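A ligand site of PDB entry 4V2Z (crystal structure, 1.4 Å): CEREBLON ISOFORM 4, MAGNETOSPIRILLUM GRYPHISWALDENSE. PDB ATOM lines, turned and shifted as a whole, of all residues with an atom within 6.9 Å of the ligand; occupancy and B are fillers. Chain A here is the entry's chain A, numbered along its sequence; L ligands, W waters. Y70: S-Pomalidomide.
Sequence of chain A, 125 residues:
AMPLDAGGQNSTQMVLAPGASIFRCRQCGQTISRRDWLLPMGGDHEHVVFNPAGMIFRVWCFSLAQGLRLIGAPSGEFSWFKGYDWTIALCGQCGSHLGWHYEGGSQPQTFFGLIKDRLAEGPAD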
ATOM      1  N   VAL A  49      27.859 -21.661  18.113  1.00  0.00           N
ATOM      2  CA  VAL A  49      26.722 -21.054  17.436  1.00  0.00           C
ATOM      3  C   VAL A  49      26.690 -21.480  15.984  1.00  0.00           C
ATOM      4  O   VAL A  49      27.728 -21.948  15.474  1.00  0.00           O
ATOM      5  CB  VAL A  49      26.807 -19.524  17.530  1.00  0.00           C
ATOM      6  CG1 VAL A  49      26.576 -19.121  19.000  1.00  0.00           C
ATOM      7  CG2 VAL A  49      28.145 -19.040  16.996  1.00  0.00           C
ATOM      8  N   PHE A  50      25.537 -21.319  15.326  1.00  0.00           N
ATOM      9  CA  PHE A  50      25.402 -21.553  13.868  1.00  0.00           C
ATOM     10  C   PHE A  50      24.794 -20.357  13.194  1.00  0.00           C
ATOM     11  O   PHE A  50      23.917 -19.703  13.805  1.00  0.00           O
ATOM     12  CB  PHE A  50      24.592 -22.795  13.459  1.00  0.00           C
ATOM     13  CG  PHE A  50      24.955 -24.048  14.171  1.00  0.00           C
ATOM     14  CD1 PHE A  50      24.563 -24.234  15.479  1.00  0.00           C
ATOM     15  CD2 PHE A  50      25.570 -25.092  13.507  1.00  0.00           C
ATOM     16  CE1 PHE A  50      24.841 -25.421  16.128  1.00  0.00           C
ATOM     17  CE2 PHE A  50      25.891 -26.269  14.169  1.00  0.00           C
ATOM     18  CZ  PHE A  50      25.523 -26.440  15.487  1.00  0.00           C
ATOM     19  N   ASN A  51      25.283 -20.075  12.021  1.00  0.00           N
ATOM     20  CA  ASN A  51      24.663 -19.070  11.171  1.00  0.00           C
ATOM     21  C   ASN A  51      23.556 -19.635  10.282  1.00  0.00           C
ATOM     22  O   ASN A  51      23.271 -20.851  10.270  1.00  0.00           O
ATOM     23  CB  ASN A  51      25.745 -18.300  10.410  1.00  0.00           C
ATOM     24  CG  ASN A  51      26.429 -19.129   9.312  1.00  0.00           C
ATOM     25  OD1 ASN A  51      25.957 -20.199   8.889  1.00  0.00           O
ATOM     26  ND2 ASN A  51      27.524 -18.573   8.776  1.00  0.00           N
ATOM     27  N   PRO A  52      22.865 -18.774   9.528  1.00  0.00           N
ATOM     28  CA  PRO A  52      21.784 -19.248   8.699  1.00  0.00           C
ATOM     29  C   PRO A  52      22.202 -20.220   7.558  1.00  0.00           C
ATOM     30  O   PRO A  52      21.345 -20.980   7.066  1.00  0.00           O
ATOM     31  CB  PRO A  52      21.146 -17.955   8.162  1.00  0.00           C
ATOM     32  CG  PRO A  52      21.599 -16.896   9.130  1.00  0.00           C
ATOM     33  CD  PRO A  52      22.913 -17.291   9.635  1.00  0.00           C
ATOM     34  N   ALA A  53      23.495 -20.280   7.279  1.00  0.00           N
ATOM     35  CA  ALA A  53      24.020 -21.220   6.238  1.00  0.00           C
ATOM     36  C   ALA A  53      24.461 -22.513   6.923  1.00  0.00           C
ATOM     37  O   ALA A  53      25.066 -23.374   6.312  1.00  0.00           O
ATOM     38  CB  ALA A  53      25.178 -20.613   5.498  1.00  0.00           C
ATOM     39  N   MET A  55      26.732 -23.073   9.192  1.00  0.00           N
ATOM     40  CA  MET A  55      28.130 -23.149   9.628  1.00  0.00           C
ATOM     41  C   MET A  55      28.159 -23.029  11.139  1.00  0.00           C
ATOM     42  O   MET A  55      27.501 -22.109  11.722  1.00  0.00           O
ATOM     43  CB  MET A  55      28.993 -22.104   8.936  1.00  0.00           C
ATOM     44  CG  MET A  55      28.866 -22.026   7.412  1.00  0.00           C
ATOM     45  SD  MET A  55      29.479 -20.429   6.813  1.00  0.00           S
ATOM     46  CE  MET A  55      31.134 -20.868   6.275  1.00  0.00           C
ATOM     47  N   PHE A  57      30.332 -22.304  14.560  1.00  0.00           N
ATOM     48  CA  PHE A  57      31.523 -21.587  15.009  1.00  0.00           C
ATOM     49  C   PHE A  57      31.721 -21.769  16.503  1.00  0.00           C
ATOM     50  O   PHE A  57      30.756 -21.671  17.298  1.00  0.00           O
ATOM     51  CB  PHE A  57      31.421 -20.130  14.742  1.00  0.00           C
ATOM     52  CG  PHE A  57      31.166 -19.751  13.291  1.00  0.00           C
ATOM     53  CD1 PHE A  57      32.197 -19.593  12.424  1.00  0.00           C
ATOM     54  CD2 PHE A  57      29.849 -19.585  12.787  1.00  0.00           C
ATOM     55  CE1 PHE A  57      31.975 -19.248  11.082  1.00  0.00           C
ATOM     56  CE2 PHE A  57      29.654 -19.276  11.467  1.00  0.00           C
ATOM     57  CZ  PHE A  57      30.683 -19.124  10.608  1.00  0.00           C
ATOM     58  N   SER A  75      24.541  -4.635  12.241  1.00  0.00           N
ATOM     59  CA  SER A  75      23.275  -5.253  12.009  1.00  0.00           C
ATOM     60  C   SER A  75      22.822  -6.083  13.219  1.00  0.00           C
ATOM     61  O   SER A  75      23.647  -6.800  13.808  1.00  0.00           O
ATOM     62  CB  SER A  75      23.370  -6.185  10.791  1.00  0.00           C
ATOM     63  OG  SER A  75      22.111  -6.713  10.609  1.00  0.00           O
ATOM     64  N   GLY A  76      21.573  -6.048  13.566  1.00  0.00           N
ATOM     65  CA  GLY A  76      21.047  -6.925  14.583  1.00  0.00           C
ATOM     66  C   GLY A  76      20.563  -8.291  14.101  1.00  0.00           C
ATOM     67  O   GLY A  76      20.203  -9.132  14.903  1.00  0.00           O
ATOM     68  N   GLU A  77      20.437  -8.438  12.786  1.00  0.00           N
ATOM     69  CA  GLU A  77      19.866  -9.607  12.171  1.00  0.00           C
ATOM     70  C   GLU A  77      20.650 -10.822  12.614  1.00  0.00           C
ATOM     71  O   GLU A  77      21.822 -10.891  12.454  1.00  0.00           O
ATOM     72  CB  GLU A  77      19.963  -9.493  10.636  1.00  0.00           C
ATOM     73  CG  GLU A  77      19.040  -8.435  10.070  1.00  0.00           C
ATOM     74  CD  GLU A  77      18.917  -8.549   8.566  1.00  0.00           C
ATOM     75  OE1 GLU A  77      18.819  -9.690   8.065  1.00  0.00           O
ATOM     76  OE2 GLU A  77      18.925  -7.492   7.888  1.00  0.00           O
ATOM     77  N   PHE A  78      19.917 -11.827  13.122  1.00  0.00           N
ATOM     78  CA  PHE A  78      20.529 -13.138  13.426  1.00  0.00           C
ATOM     79  C   PHE A  78      21.491 -13.121  14.590  1.00  0.00           C
ATOM     80  O   PHE A  78      22.266 -14.022  14.772  1.00  0.00           O
ATOM     81  CB  PHE A  78      21.174 -13.776  12.210  1.00  0.00           C
ATOM     82  CG  PHE A  78      20.253 -13.945  11.045  1.00  0.00           C
ATOM     83  CD1 PHE A  78      19.275 -14.856  11.088  1.00  0.00           C
ATOM     84  CD2 PHE A  78      20.427 -13.154   9.916  1.00  0.00           C
ATOM     85  CE1 PHE A  78      18.405 -15.007  10.016  1.00  0.00           C
ATOM     86  CE2 PHE A  78      19.562 -13.283   8.851  1.00  0.00           C
ATOM     87  CZ  PHE A  78      18.585 -14.224   8.897  1.00  0.00           C
ATOM     88  N   SER A  79      21.559 -12.003  15.333  1.00  0.00           N
ATOM     89  CA  SER A  79      22.544 -11.882  16.361  1.00  0.00           C
ATOM     90  C   SER A  79      22.456 -12.984  17.404  1.00  0.00           C
ATOM     91  O   SER A  79      21.408 -13.282  17.916  1.00  0.00           O
ATOM     92  CB  SER A  79      22.484 -10.527  17.082  1.00  0.00           C
ATOM     93  OG  SER A  79      23.542 -10.448  17.996  1.00  0.00           O
ATOM     94  N   TRP A  80      23.642 -13.545  17.661  1.00  0.00           N
ATOM     95  CA  TRP A  80      23.810 -14.622  18.670  1.00  0.00           C
ATOM     96  C   TRP A  80      23.797 -14.109  20.106  1.00  0.00           C
ATOM     97  O   TRP A  80      23.606 -14.869  21.035  1.00  0.00           O
ATOM     98  CB  TRP A  80      25.086 -15.418  18.482  1.00  0.00           C
ATOM     99  CG  TRP A  80      25.131 -16.169  17.189  1.00  0.00           C
ATOM    100  CD1 TRP A  80      24.166 -16.999  16.715  1.00  0.00           C
ATOM    101  CD2 TRP A  80      26.186 -16.175  16.277  1.00  0.00           C
ATOM    102  NE1 TRP A  80      24.564 -17.550  15.480  1.00  0.00           N
ATOM    103  CE2 TRP A  80      25.806 -17.026  15.185  1.00  0.00           C
ATOM    104  CE3 TRP A  80      27.421 -15.555  16.224  1.00  0.00           C
ATOM    105  CZ2 TRP A  80      26.665 -17.262  14.121  1.00  0.00           C
ATOM    106  CZ3 TRP A  80      28.250 -15.761  15.145  1.00  0.00           C
ATOM    107  CH2 TRP A  80      27.873 -16.640  14.100  1.00  0.00           C
ATOM    108  N   PHE A  81      23.861 -12.804  20.305  1.00  0.00           N
ATOM    109  CA  PHE A  81      24.010 -12.233  21.639  1.00  0.00           C
ATOM    110  C   PHE A  81      22.904 -11.202  21.795  1.00  0.00           C
ATOM    111  O   PHE A  81      22.892 -10.206  21.128  1.00  0.00           O
ATOM    112  CB  PHE A  81      25.420 -11.658  21.884  1.00  0.00           C
ATOM    113  CG  PHE A  81      26.540 -12.671  21.736  1.00  0.00           C
ATOM    114  CD1 PHE A  81      26.913 -13.433  22.876  1.00  0.00           C
ATOM    115  CD2 PHE A  81      27.180 -12.838  20.595  1.00  0.00           C
ATOM    116  CE1 PHE A  81      27.958 -14.360  22.808  1.00  0.00           C
ATOM    117  CE2 PHE A  81      28.225 -13.768  20.469  1.00  0.00           C
ATOM    118  CZ  PHE A  81      28.583 -14.548  21.602  1.00  0.00           C
ATOM    119  N   TYR A  84      22.759  -7.093  21.147  1.00  0.00           N
ATOM    120  CA  TYR A  84      23.923  -6.628  20.386  1.00  0.00           C
ATOM    121  C   TYR A  84      23.759  -6.693  18.893  1.00  0.00           C
ATOM    122  O   TYR A  84      23.113  -7.591  18.361  1.00  0.00           O
ATOM    123  CB  TYR A  84      25.217  -7.417  20.732  1.00  0.00           C
ATOM    124  CG  TYR A  84      25.612  -7.329  22.153  1.00  0.00           C
ATOM    125  CD1 TYR A  84      25.155  -8.217  23.066  1.00  0.00           C
ATOM    126  CD2 TYR A  84      26.499  -6.352  22.592  1.00  0.00           C
ATOM    127  CE1 TYR A  84      25.513  -8.114  24.429  1.00  0.00           C
ATOM    128  CE2 TYR A  84      26.902  -6.258  23.869  1.00  0.00           C
ATOM    129  CZ  TYR A  84      26.394  -7.160  24.805  1.00  0.00           C
ATOM    130  OH  TYR A  84      26.700  -7.064  26.153  1.00  0.00           O
ATOM    131  N   TRP A  86      26.038  -6.567  15.241  1.00  0.00           N
ATOM    132  CA  TRP A  86      27.372  -7.060  14.809  1.00  0.00           C
ATOM    133  C   TRP A  86      27.891  -6.436  13.550  1.00  0.00           C
ATOM    134  O   TRP A  86      27.097  -6.065  12.712  1.00  0.00           O
ATOM    135  CB  TRP A  86      27.357  -8.570  14.653  1.00  0.00           C
ATOM    136  CG  TRP A  86      26.322  -9.126  13.789  1.00  0.00           C
ATOM    137  CD1 TRP A  86      25.068  -9.613  14.149  1.00  0.00           C
ATOM    138  CD2 TRP A  86      26.364  -9.183  12.334  1.00  0.00           C
ATOM    139  NE1 TRP A  86      24.392  -9.964  13.034  1.00  0.00           N
ATOM    140  CE2 TRP A  86      25.118  -9.705  11.915  1.00  0.00           C
ATOM    141  CE3 TRP A  86      27.336  -8.902  11.352  1.00  0.00           C
ATOM    142  CZ2 TRP A  86      24.802  -9.909  10.569  1.00  0.00           C
ATOM    143  CZ3 TRP A  86      26.985  -9.089   9.992  1.00  0.00           C
ATOM    144  CH2 TRP A  86      25.775  -9.641   9.618  1.00  0.00           C
ATOM    145  N   THR A  87      29.245  -6.423  13.453  1.00  0.00           N
ATOM    146  CA  THR A  87      29.989  -6.077  12.263  1.00  0.00           C
ATOM    147  C   THR A  87      30.942  -7.199  12.049  1.00  0.00           C
ATOM    148  O   THR A  87      31.526  -7.687  12.987  1.00  0.00           O
ATOM    149  CB  THR A  87      30.697  -4.727  12.307  1.00  0.00           C
ATOM    150  OG1 THR A  87      31.667  -4.697  13.335  1.00  0.00           O
ATOM    151  CG2 THR A  87      29.632  -3.667  12.683  1.00  0.00           C
ATOM    152  N   ILE A  88      31.180  -7.584  10.800  1.00  0.00           N
ATOM    153  CA  ILE A  88      32.208  -8.602  10.458  1.00  0.00           C
ATOM    154  C   ILE A  88      33.581  -8.039  10.828  1.00  0.00           C
ATOM    155  O   ILE A  88      33.872  -6.848  10.534  1.00  0.00           O
ATOM    156  CB  ILE A  88      32.091  -8.893   8.987  1.00  0.00           C
ATOM    157  CG1 ILE A  88      30.872  -9.696   8.729  1.00  0.00           C
ATOM    158  CG2 ILE A  88      33.346  -9.612   8.457  1.00  0.00           C
ATOM    159  CD1 ILE A  88      30.475  -9.749   7.255  1.00  0.00           C
ATOM    160  N   HIS A  97      38.499 -14.004   7.714  1.00  0.00           N
ATOM    161  CA  HIS A  97      37.388 -13.711   8.568  1.00  0.00           C
ATOM    162  C   HIS A  97      37.619 -14.300   9.942  1.00  0.00           C
ATOM    163  O   HIS A  97      37.572 -15.523  10.176  1.00  0.00           O
ATOM    164  CB  HIS A  97      36.100 -14.279   8.024  1.00  0.00           C
ATOM    165  CG  HIS A  97      34.945 -14.032   8.875  1.00  0.00           C
ATOM    166  ND1 HIS A  97      33.862 -14.892   8.875  1.00  0.00           N
ATOM    167  CD2 HIS A  97      34.682 -13.073   9.783  1.00  0.00           C
ATOM    168  CE1 HIS A  97      32.982 -14.453   9.743  1.00  0.00           C
ATOM    169  NE2 HIS A  97      33.450 -13.345  10.306  1.00  0.00           N
ATOM    170  N   TRP A 100      33.543 -11.361  14.700  1.00  0.00           N
ATOM    171  CA  TRP A 100      32.599 -10.209  14.683  1.00  0.00           C
ATOM    172  C   TRP A 100      32.890  -9.270  15.823  1.00  0.00           C
ATOM    173  O   TRP A 100      33.325  -9.736  16.909  1.00  0.00           O
ATOM    174  CB  TRP A 100      31.140 -10.694  14.781  1.00  0.00           C
ATOM    175  CG  TRP A 100      30.744 -11.660  13.655  1.00  0.00           C
ATOM    176  CD1 TRP A 100      30.192 -11.359  12.424  1.00  0.00           C
ATOM    177  CD2 TRP A 100      30.950 -13.060  13.616  1.00  0.00           C
ATOM    178  NE1 TRP A 100      30.076 -12.455  11.693  1.00  0.00           N
ATOM    179  CE2 TRP A 100      30.504 -13.529  12.391  1.00  0.00           C
ATOM    180  CE3 TRP A 100      31.512 -13.979  14.514  1.00  0.00           C
ATOM    181  CZ2 TRP A 100      30.527 -14.891  12.031  1.00  0.00           C
ATOM    182  CZ3 TRP A 100      31.616 -15.345  14.117  1.00  0.00           C
ATOM    183  CH2 TRP A 100      31.119 -15.761  12.900  1.00  0.00           C
ATOM    184  N   TYR A 102      30.765  -6.828  18.299  1.00  0.00           N
ATOM    185  CA  TYR A 102      29.418  -6.577  18.824  1.00  0.00           C
ATOM    186  C   TYR A 102      29.332  -5.229  19.556  1.00  0.00           C
ATOM    187  O   TYR A 102      30.270  -4.868  20.244  1.00  0.00           O
ATOM    188  CB  TYR A 102      29.046  -7.712  19.747  1.00  0.00           C
ATOM    189  CG  TYR A 102      28.821  -9.013  19.004  1.00  0.00           C
ATOM    190  CD1 TYR A 102      27.557  -9.278  18.450  1.00  0.00           C
ATOM    191  CD2 TYR A 102      29.841  -9.916  18.822  1.00  0.00           C
ATOM    192  CE1 TYR A 102      27.357 -10.450  17.771  1.00  0.00           C
ATOM    193  CE2 TYR A 102      29.647 -11.076  18.128  1.00  0.00           C
ATOM    194  CZ  TYR A 102      28.443 -11.296  17.500  1.00  0.00           C
ATOM    195  OH  TYR A 102      28.228 -12.507  16.836  1.00  0.00           O
HETATM  196  C1  Y70 L   1      24.282 -15.000   6.045  1.00  0.00           C
HETATM  197  C2  Y70 L   1      25.465 -15.742   5.930  1.00  0.00           C
HETATM  198  C3  Y70 L   1      26.316 -15.874   7.005  1.00  0.00           C
HETATM  199  C4  Y70 L   1      25.990 -15.243   8.200  1.00  0.00           C
HETATM  200  C5  Y70 L   1      24.845 -14.512   8.322  1.00  0.00           C
HETATM  201  C6  Y70 L   1      23.947 -14.388   7.262  1.00  0.00           C
HETATM  202  C7  Y70 L   1      26.632 -15.165   9.416  1.00  0.00           C
HETATM  203  N8  Y70 L   1      25.950 -14.430  10.301  1.00  0.00           N
HETATM  204  C9  Y70 L   1      24.891 -14.090   9.640  1.00  0.00           C
HETATM  205  N10 Y70 L   1      22.783 -13.676   7.347  1.00  0.00           N
HETATM  206  O11 Y70 L   1      23.956 -13.294  10.220  1.00  0.00           O
HETATM  207  C12 Y70 L   1      26.283 -14.310  11.708  1.00  0.00           C
HETATM  208  O13 Y70 L   1      27.824 -15.803   9.803  1.00  0.00           O
HETATM  209  C14 Y70 L   1      26.678 -12.877  11.975  1.00  0.00           C
HETATM  210  C15 Y70 L   1      25.171 -14.699  12.650  1.00  0.00           C
HETATM  211  N16 Y70 L   1      24.996 -14.136  13.840  1.00  0.00           N
HETATM  212  C17 Y70 L   1      25.855 -13.234  14.369  1.00  0.00           C
HETATM  213  C18 Y70 L   1      26.950 -12.742  13.451  1.00  0.00           C
HETATM  214  O19 Y70 L   1      24.363 -15.681  12.295  1.00  0.00           O
HETATM  215  O20 Y70 L   1      25.753 -12.879  15.526  1.00  0.00           O
HETATM  216  O   HOH W   1      28.832 -12.602   8.944  1.00  0.00           O
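Residues that only touch the ligand: Pro 52 (3.4 Å), Glu 77 (3.9 Å), Ser 79 (3.5 Å), Trp 86 (3.5 Å) and Trp 100 (3.4 Å). Hydrophobic or aromatic side chains that line the ligand: Pro 52, Phe 78, Trp 80, Trp 86, Trp 100 and Tyr 102. Of the 21 residues printed, 9 come within 4 Å of the ligand. Along chain A the residues within 4 Å of the ligand span positions 51 to 102. The nearest printed residue that does not touch the ligand is Phe 57 (4.3 Å).
The side-chain amide oxygen of Asn 51 lies within hydrogen-bond range of the backbone NH of Met 55 (3.0 Å). The indole nitrogen (NE1) of Trp 86 is in hydrogen-bond range of the backbone carbonyl oxygen (O) of Glu 77 (2.8 Å). The backbone NH (N) of Trp 86 lies within hydrogen-bond range of the backbone carbonyl oxygen (O) of Ser 75, at 2.8 Å. The backbone NH (N) of Ala 53 sits at hydrogen-bond distance from the side-chain amide oxygen (OD1) of Asn 51 (2.9 Å). The side-chain hydroxyl of Ser 79 lies within hydrogen-bond range of the backbone carbonyl oxygen of Tyr 84 (2.9 Å). NE1 of Trp 80 lies within hydrogen-bond range of O of Phe 50, 2.8 Å away. The backbone NH (N) of Glu 77 is in hydrogen-bond range of the side-chain hydroxyl (OG) of Ser 75 (3.2 Å). O of Phe 81 sits at hydrogen-bond distance from OG of Ser 79.
N of Trp 80 sits at hydrogen-bond distance from O20 of the ligand, at 3.1 Å. An oxygen (O13) of the ligand sits at hydrogen-bond distance from the side-chain amide nitrogen (ND2) of Asn 51, 3.0 Å away. O of Phe 78 lies within hydrogen-bond range of N16 of the ligand, at 2.9 Å. The side-chain hydroxyl (OH) of Tyr 102 is in hydrogen-bond range of an oxygen (O20) of the ligand (2.8 Å).
Water W1 lies within hydrogen-bond range of NE1 of Trp 100 (3.0 Å) and O13 of the ligand (3.5 Å).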
